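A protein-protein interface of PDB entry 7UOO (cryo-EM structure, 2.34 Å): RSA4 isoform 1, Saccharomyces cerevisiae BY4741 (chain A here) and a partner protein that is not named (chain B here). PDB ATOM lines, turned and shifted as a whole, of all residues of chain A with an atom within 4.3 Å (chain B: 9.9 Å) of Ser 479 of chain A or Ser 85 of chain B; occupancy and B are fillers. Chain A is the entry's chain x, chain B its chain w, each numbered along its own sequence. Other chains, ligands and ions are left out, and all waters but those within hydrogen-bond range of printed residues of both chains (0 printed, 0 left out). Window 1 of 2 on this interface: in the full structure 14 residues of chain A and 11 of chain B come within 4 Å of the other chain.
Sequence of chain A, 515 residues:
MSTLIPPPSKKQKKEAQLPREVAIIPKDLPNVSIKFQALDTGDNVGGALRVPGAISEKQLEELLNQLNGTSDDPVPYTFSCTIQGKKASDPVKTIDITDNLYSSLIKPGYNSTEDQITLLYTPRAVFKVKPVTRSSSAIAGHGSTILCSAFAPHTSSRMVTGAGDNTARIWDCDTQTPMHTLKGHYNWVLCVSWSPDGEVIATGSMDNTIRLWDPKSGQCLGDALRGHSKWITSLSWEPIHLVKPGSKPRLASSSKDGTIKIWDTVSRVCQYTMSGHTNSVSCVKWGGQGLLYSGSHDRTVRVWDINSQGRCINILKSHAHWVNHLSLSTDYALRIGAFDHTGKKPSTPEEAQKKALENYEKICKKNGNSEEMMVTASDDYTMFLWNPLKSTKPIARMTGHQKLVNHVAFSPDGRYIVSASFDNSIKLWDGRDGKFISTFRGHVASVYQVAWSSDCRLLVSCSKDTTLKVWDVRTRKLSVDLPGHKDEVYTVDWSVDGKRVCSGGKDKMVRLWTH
Of chain B, only Thr 74 (3.8 Å) and Ser 85 (3.0 Å) come within 4 Å of Ser 479 of chain A. Of the printed residues of chain A, Ser 85 of chain B touches Ser 479 (3.0 Å) and Val 480 (3.7 Å). Leu 478 of chain A touches just one residue of chain B: Thr 74. Val 480 of chain A touches three residues of chain B. Printed residues of chain A within 4 Å of Ser 76 of chain B: Val 480. Printed residues of chain A within 4 Å of Thr 74 of chain B: Leu 478 (3.6 Å), Ser 479 (3.8 Å) and Val 480 (3.4 Å). Thr 72 of chain B touches none of the printed residues of chain A. The nearest residue of chain B that does not touch Ser 479 of chain A is Thr 73 of chain B (4.4 Å). The nearest printed residue of chain A that does not touch Ser 85 of chain B is Leu 478 of chain A (6.3 Å). The nearest printed residue of chain A that does not touch Thr 74 of chain B is Lys 477 of chain A (6.6 Å).
Among the printed residues, merely in contact across the chains: Leu 478 of chain A with Thr 74 of chain B (3.6 Å), Ser 479 of chain A with Thr 74 of chain B (3.8 Å), Val 480 of chain A with Thr 74 of chain B (3.4 Å), Val 480 of chain A with Ser 76 of chain B (3.5 Å) and Val 480 of chain A with Ser 85 of chain B (3.7 Å).
The side-chain hydroxyl of Ser 85 of chain B sits at hydrogen-bond distance from the backbone carbonyl oxygen of Ser 479 of chain A (3.0 Å).
The backbone carbonyl oxygen of Val 480 of chain A sits at hydrogen-bond distance from the backbone NH of Val 470 of chain A (2.9 Å). The backbone carbonyl oxygen of Val 470 of chain A lies within hydrogen-bond range of the backbone NH of Ser 479 of chain A, 2.7 Å away. The backbone carbonyl oxygen of Glu 75 of chain B lies within hydrogen-bond range of the backbone NH of Ser 85 of chain B, at 3.1 Å.
Printed residues of chain B that touch a printed residue of chain A: Thr 74, Ser 76 and Ser 85. Of the 7 printed residues of chain A, 3 touch a printed residue of chain B. Printed residues of chain A that touch a printed residue of chain B: Leu 478, Ser 479 and Val 480. Among the printed residues, no Asp or Glu carboxylate lies within 4 Å of a Lys or Arg side-chain nitrogen of the other chain.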
ATOM      1  N   VAL A 470     -21.059 -30.804  -9.883  1.00  0.00           N
ATOM      2  CA  VAL A 470     -21.211 -31.776  -8.811  1.00  0.00           C
ATOM      3  C   VAL A 470     -22.372 -31.333  -7.936  1.00  0.00           C
ATOM      4  O   VAL A 470     -22.393 -30.196  -7.447  1.00  0.00           O
ATOM      5  CB  VAL A 470     -19.920 -31.915  -7.988  1.00  0.00           C
ATOM      6  CG1 VAL A 470     -20.091 -32.954  -6.898  1.00  0.00           C
ATOM      7  CG2 VAL A 470     -18.754 -32.270  -8.887  1.00  0.00           C
ATOM      8  N   TRP A 471     -23.333 -32.233  -7.753  1.00  0.00           N
ATOM      9  CA  TRP A 471     -24.538 -32.008  -6.973  1.00  0.00           C
ATOM     10  C   TRP A 471     -24.516 -32.885  -5.729  1.00  0.00           C
ATOM     11  O   TRP A 471     -24.053 -34.031  -5.773  1.00  0.00           O
ATOM     12  CB  TRP A 471     -25.796 -32.331  -7.786  1.00  0.00           C
ATOM     13  CG  TRP A 471     -25.763 -31.855  -9.208  1.00  0.00           C
ATOM     14  CD1 TRP A 471     -25.181 -32.483 -10.269  1.00  0.00           C
ATOM     15  CD2 TRP A 471     -26.351 -30.659  -9.725  1.00  0.00           C
ATOM     16  NE1 TRP A 471     -25.361 -31.748 -11.412  1.00  0.00           N
ATOM     17  CE2 TRP A 471     -26.081 -30.623 -11.106  1.00  0.00           C
ATOM     18  CE3 TRP A 471     -27.084 -29.615  -9.155  1.00  0.00           C
ATOM     19  CZ2 TRP A 471     -26.512 -29.583 -11.923  1.00  0.00           C
ATOM     20  CZ3 TRP A 471     -27.507 -28.583  -9.967  1.00  0.00           C
ATOM     21  CH2 TRP A 471     -27.220 -28.575 -11.335  1.00  0.00           C
ATOM     22  N   ASP A 472     -25.021 -32.338  -4.626  1.00  0.00           N
ATOM     23  CA  ASP A 472     -25.233 -33.091  -3.397  1.00  0.00           C
ATOM     24  C   ASP A 472     -26.646 -33.660  -3.418  1.00  0.00           C
ATOM     25  O   ASP A 472     -27.623 -32.904  -3.467  1.00  0.00           O
ATOM     26  CB  ASP A 472     -25.026 -32.194  -2.178  1.00  0.00           C
ATOM     27  CG  ASP A 472     -25.165 -32.942  -0.865  1.00  0.00           C
ATOM     28  OD1 ASP A 472     -25.090 -34.189  -0.869  1.00  0.00           O
ATOM     29  OD2 ASP A 472     -25.350 -32.279   0.177  1.00  0.00           O
ATOM     30  N   LYS A 477     -29.082 -29.851  -4.065  1.00  0.00           N
ATOM     31  CA  LYS A 477     -28.622 -28.565  -4.563  1.00  0.00           C
ATOM     32  C   LYS A 477     -27.279 -28.746  -5.257  1.00  0.00           C
ATOM     33  O   LYS A 477     -26.648 -29.803  -5.178  1.00  0.00           O
ATOM     34  CB  LYS A 477     -28.505 -27.535  -3.436  1.00  0.00           C
ATOM     35  CG  LYS A 477     -27.502 -27.919  -2.365  1.00  0.00           C
ATOM     36  CD  LYS A 477     -27.485 -26.913  -1.230  1.00  0.00           C
ATOM     37  CE  LYS A 477     -26.503 -27.333  -0.147  1.00  0.00           C
ATOM     38  NZ  LYS A 477     -25.116 -27.462  -0.668  1.00  0.00           N
ATOM     39  N   LEU A 478     -26.844 -27.693  -5.945  1.00  0.00           N
ATOM     40  CA  LEU A 478     -25.553 -27.707  -6.618  1.00  0.00           C
ATOM     41  C   LEU A 478     -24.432 -27.569  -5.598  1.00  0.00           C
ATOM     42  O   LEU A 478     -24.391 -26.595  -4.839  1.00  0.00           O
ATOM     43  CB  LEU A 478     -25.483 -26.580  -7.644  1.00  0.00           C
ATOM     44  CG  LEU A 478     -24.120 -26.333  -8.286  1.00  0.00           C
ATOM     45  CD1 LEU A 478     -23.797 -27.421  -9.294  1.00  0.00           C
ATOM     46  CD2 LEU A 478     -24.080 -24.963  -8.935  1.00  0.00           C
ATOM     47  N   SER A 479     -23.520 -28.541  -5.581  1.00  0.00           N
ATOM     48  CA  SER A 479     -22.399 -28.483  -4.652  1.00  0.00           C
ATOM     49  C   SER A 479     -21.271 -27.620  -5.206  1.00  0.00           C
ATOM     50  O   SER A 479     -20.839 -26.660  -4.561  1.00  0.00           O
ATOM     51  CB  SER A 479     -21.901 -29.895  -4.330  1.00  0.00           C
ATOM     52  OG  SER A 479     -20.894 -29.866  -3.332  1.00  0.00           O
ATOM     53  N   VAL A 480     -20.787 -27.933  -6.408  1.00  0.00           N
ATOM     54  CA  VAL A 480     -19.692 -27.159  -6.988  1.00  0.00           C
ATOM     55  C   VAL A 480     -19.817 -27.146  -8.508  1.00  0.00           C
ATOM     56  O   VAL A 480     -20.327 -28.087  -9.124  1.00  0.00           O
ATOM     57  CB  VAL A 480     -18.311 -27.690  -6.519  1.00  0.00           C
ATOM     58  CG1 VAL A 480     -17.956 -28.995  -7.194  1.00  0.00           C
ATOM     59  CG2 VAL A 480     -17.217 -26.650  -6.744  1.00  0.00           C
ATOM     60  N   LYS B  71     -22.408 -17.452   4.726  1.00  0.00           N
ATOM     61  CA  LYS B  71     -22.400 -17.377   3.274  1.00  0.00           C
ATOM     62  C   LYS B  71     -21.622 -18.557   2.713  1.00  0.00           C
ATOM     63  O   LYS B  71     -20.501 -18.839   3.159  1.00  0.00           O
ATOM     64  CB  LYS B  71     -21.778 -16.062   2.797  1.00  0.00           C
ATOM     65  CG  LYS B  71     -21.524 -16.010   1.299  1.00  0.00           C
ATOM     66  CD  LYS B  71     -20.904 -14.689   0.879  1.00  0.00           C
ATOM     67  CE  LYS B  71     -20.642 -14.665  -0.615  1.00  0.00           C
ATOM     68  NZ  LYS B  71     -21.891 -14.879  -1.396  1.00  0.00           N
ATOM     69  N   THR B  72     -22.229 -19.245   1.748  1.00  0.00           N
ATOM     70  CA  THR B  72     -21.607 -20.324   0.999  1.00  0.00           C
ATOM     71  C   THR B  72     -21.613 -19.968  -0.482  1.00  0.00           C
ATOM     72  O   THR B  72     -22.425 -19.163  -0.943  1.00  0.00           O
ATOM     73  CB  THR B  72     -22.338 -21.659   1.210  1.00  0.00           C
ATOM     74  OG1 THR B  72     -23.608 -21.621   0.550  1.00  0.00           O
ATOM     75  CG2 THR B  72     -22.557 -21.925   2.689  1.00  0.00           C
ATOM     76  N   THR B  73     -20.697 -20.579  -1.227  1.00  0.00           N
ATOM     77  CA  THR B  73     -20.602 -20.355  -2.661  1.00  0.00           C
ATOM     78  C   THR B  73     -20.356 -21.687  -3.353  1.00  0.00           C
ATOM     79  O   THR B  73     -20.058 -22.697  -2.713  1.00  0.00           O
ATOM     80  CB  THR B  73     -19.490 -19.356  -3.012  1.00  0.00           C
ATOM     81  OG1 THR B  73     -19.550 -19.039  -4.407  1.00  0.00           O
ATOM     82  CG2 THR B  73     -18.133 -19.943  -2.696  1.00  0.00           C
ATOM     83  N   THR B  74     -20.497 -21.684  -4.677  1.00  0.00           N
ATOM     84  CA  THR B  74     -20.289 -22.882  -5.477  1.00  0.00           C
ATOM     85  C   THR B  74     -19.116 -22.764  -6.440  1.00  0.00           C
ATOM     86  O   THR B  74     -18.833 -23.724  -7.164  1.00  0.00           O
ATOM     87  CB  THR B  74     -21.560 -23.232  -6.261  1.00  0.00           C
ATOM     88  OG1 THR B  74     -21.858 -22.185  -7.194  1.00  0.00           O
ATOM     89  CG2 THR B  74     -22.737 -23.412  -5.318  1.00  0.00           C
ATOM     90  N   GLU B  75     -18.433 -21.624  -6.479  1.00  0.00           N
ATOM     91  CA  GLU B  75     -17.294 -21.488  -7.373  1.00  0.00           C
ATOM     92  C   GLU B  75     -16.109 -22.293  -6.849  1.00  0.00           C
ATOM     93  O   GLU B  75     -15.942 -22.488  -5.642  1.00  0.00           O
ATOM     94  CB  GLU B  75     -16.909 -20.017  -7.549  1.00  0.00           C
ATOM     95  CG  GLU B  75     -16.275 -19.369  -6.337  1.00  0.00           C
ATOM     96  CD  GLU B  75     -15.770 -17.967  -6.626  1.00  0.00           C
ATOM     97  OE1 GLU B  75     -15.941 -17.496  -7.769  1.00  0.00           O
ATOM     98  OE2 GLU B  75     -15.204 -17.335  -5.708  1.00  0.00           O
ATOM     99  N   SER B  76     -15.292 -22.777  -7.777  1.00  0.00           N
ATOM    100  CA  SER B  76     -14.166 -23.622  -7.422  1.00  0.00           C
ATOM    101  C   SER B  76     -12.962 -22.774  -7.025  1.00  0.00           C
ATOM    102  O   SER B  76     -12.996 -21.542  -7.035  1.00  0.00           O
ATOM    103  CB  SER B  76     -13.811 -24.545  -8.584  1.00  0.00           C
ATOM    104  OG  SER B  76     -14.935 -25.307  -8.980  1.00  0.00           O
ATOM    105  N   VAL B  77     -11.879 -23.462  -6.660  1.00  0.00           N
ATOM    106  CA  VAL B  77     -10.647 -22.769  -6.309  1.00  0.00           C
ATOM    107  C   VAL B  77      -9.972 -22.234  -7.568  1.00  0.00           C
ATOM    108  O   VAL B  77     -10.320 -22.585  -8.701  1.00  0.00           O
ATOM    109  CB  VAL B  77      -9.708 -23.699  -5.526  1.00  0.00           C
ATOM    110  CG1 VAL B  77     -10.476 -24.439  -4.446  1.00  0.00           C
ATOM    111  CG2 VAL B  77      -9.034 -24.673  -6.469  1.00  0.00           C
ATOM    112  N   GLY B  78      -8.989 -21.363  -7.361  1.00  0.00           N
ATOM    113  CA  GLY B  78      -8.236 -20.814  -8.467  1.00  0.00           C
ATOM    114  C   GLY B  78      -8.914 -19.688  -9.209  1.00  0.00           C
ATOM    115  O   GLY B  78      -8.380 -19.224 -10.223  1.00  0.00           O
ATOM    116  N   GLY B  79     -10.073 -19.235  -8.741  1.00  0.00           N
ATOM    117  CA  GLY B  79     -10.775 -18.115  -9.336  1.00  0.00           C
ATOM    118  C   GLY B  79     -10.734 -16.914  -8.411  1.00  0.00           C
ATOM    119  O   GLY B  79     -10.473 -17.047  -7.214  1.00  0.00           O
ATOM    120  N   GLY B  81     -11.842 -13.974  -6.001  1.00  0.00           N
ATOM    121  CA  GLY B  81     -12.865 -13.842  -4.981  1.00  0.00           C
ATOM    122  C   GLY B  81     -12.416 -14.280  -3.603  1.00  0.00           C
ATOM    123  O   GLY B  81     -12.799 -13.675  -2.598  1.00  0.00           O
ATOM    124  N   GLY B  82     -11.602 -15.332  -3.539  1.00  0.00           N
ATOM    125  CA  GLY B  82     -11.034 -15.793  -2.295  1.00  0.00           C
ATOM    126  C   GLY B  82     -11.865 -16.806  -1.536  1.00  0.00           C
ATOM    127  O   GLY B  82     -11.329 -17.486  -0.654  1.00  0.00           O
ATOM    128  N   GLN B  83     -13.150 -16.938  -1.848  1.00  0.00           N
ATOM    129  CA  GLN B  83     -14.017 -17.907  -1.187  1.00  0.00           C
ATOM    130  C   GLN B  83     -14.292 -19.056  -2.145  1.00  0.00           C
ATOM    131  O   GLN B  83     -14.827 -18.844  -3.238  1.00  0.00           O
ATOM    132  CB  GLN B  83     -15.327 -17.266  -0.732  1.00  0.00           C
ATOM    133  CG  GLN B  83     -16.248 -18.239  -0.016  1.00  0.00           C
ATOM    134  CD  GLN B  83     -17.561 -17.612   0.405  1.00  0.00           C
ATOM    135  OE1 GLN B  83     -17.869 -16.480   0.034  1.00  0.00           O
ATOM    136  NE2 GLN B  83     -18.343 -18.348   1.184  1.00  0.00           N
ATOM    137  N   SER B  84     -13.927 -20.264  -1.734  1.00  0.00           N
ATOM    138  CA  SER B  84     -14.159 -21.460  -2.523  1.00  0.00           C
ATOM    139  C   SER B  84     -15.396 -22.188  -2.005  1.00  0.00           C
ATOM    140  O   SER B  84     -16.052 -21.756  -1.055  1.00  0.00           O
ATOM    141  CB  SER B  84     -12.929 -22.368  -2.498  1.00  0.00           C
ATOM    142  OG  SER B  84     -12.678 -22.852  -1.192  1.00  0.00           O
ATOM    143  N   SER B  85     -15.705 -23.319  -2.643  1.00  0.00           N
ATOM    144  CA  SER B  85     -16.931 -24.049  -2.336  1.00  0.00           C
ATOM    145  C   SER B  85     -16.928 -24.586  -0.910  1.00  0.00           C
ATOM    146  O   SER B  85     -17.964 -24.578  -0.235  1.00  0.00           O
ATOM    147  CB  SER B  85     -17.117 -25.189  -3.337  1.00  0.00           C
ATOM    148  OG  SER B  85     -18.341 -25.865  -3.122  1.00  0.00           O
ATOM    149  N   VAL B  86     -15.776 -25.062  -0.434  1.00  0.00           N
ATOM    150  CA  VAL B  86     -15.709 -25.652   0.899  1.00  0.00           C
ATOM    151  C   VAL B  86     -15.738 -24.607   2.009  1.00  0.00           C
ATOM    152  O   VAL B  86     -16.108 -24.933   3.142  1.00  0.00           O
ATOM    153  CB  VAL B  86     -14.454 -26.527   1.040  1.00  0.00           C
ATOM    154  CG1 VAL B  86     -14.543 -27.728   0.113  1.00  0.00           C
ATOM    155  CG2 VAL B  86     -13.203 -25.714   0.746  1.00  0.00           C
ATOM    156  N   MET B  87     -15.365 -23.364   1.719  1.00  0.00           N
ATOM    157  CA  MET B  87     -15.315 -22.329   2.741  1.00  0.00           C
ATOM    158  C   MET B  87     -16.710 -21.783   3.019  1.00  0.00           C
ATOM    159  O   MET B  87     -17.465 -21.474   2.091  1.00  0.00           O
ATOM    160  CB  MET B  87     -14.385 -21.198   2.303  1.00  0.00           C
ATOM    161  CG  MET B  87     -12.977 -21.648   1.958  1.00  0.00           C
ATOM    162  SD  MET B  87     -12.008 -20.334   1.192  1.00  0.00           S
ATOM    163  CE  MET B  87     -12.037 -19.092   2.481  1.00  0.00           C
ATOM    164  N   THR B  88     -17.052 -21.673   4.300  1.00  0.00           N
ATOM    165  CA  THR B  88     -18.276 -21.025   4.753  1.00  0.00           C
ATOM    166  C   THR B  88     -17.888 -19.822   5.601  1.00  0.00           C
ATOM    167  O   THR B  88     -17.133 -19.964   6.569  1.00  0.00           O
ATOM    168  CB  THR B  88     -19.148 -21.990   5.560  1.00  0.00           C
ATOM    169  OG1 THR B  88     -19.286 -23.225   4.846  1.00  0.00           O
ATOM    170  CG2 THR B  88     -20.523 -21.401   5.784  1.00  0.00           C
ATOM    171  N   LEU B  89     -18.393 -18.645   5.244  1.00  0.00           N
ATOM    172  CA  LEU B  89     -17.931 -17.397   5.841  1.00  0.00           C
ATOM    173  C   LEU B  89     -19.029 -16.758   6.680  1.00  0.00           C
ATOM    174  O   LEU B  89     -20.170 -16.646   6.232  1.00  0.00           O
ATOM    175  CB  LEU B  89     -17.468 -16.417   4.762  1.00  0.00           C
ATOM    176  CG  LEU B  89     -16.267 -16.845   3.920  1.00  0.00           C
ATOM    177  CD1 LEU B  89     -15.886 -15.749   2.942  1.00  0.00           C
ATOM    178  CD2 LEU B  89     -15.091 -17.207   4.810  1.00  0.00           C
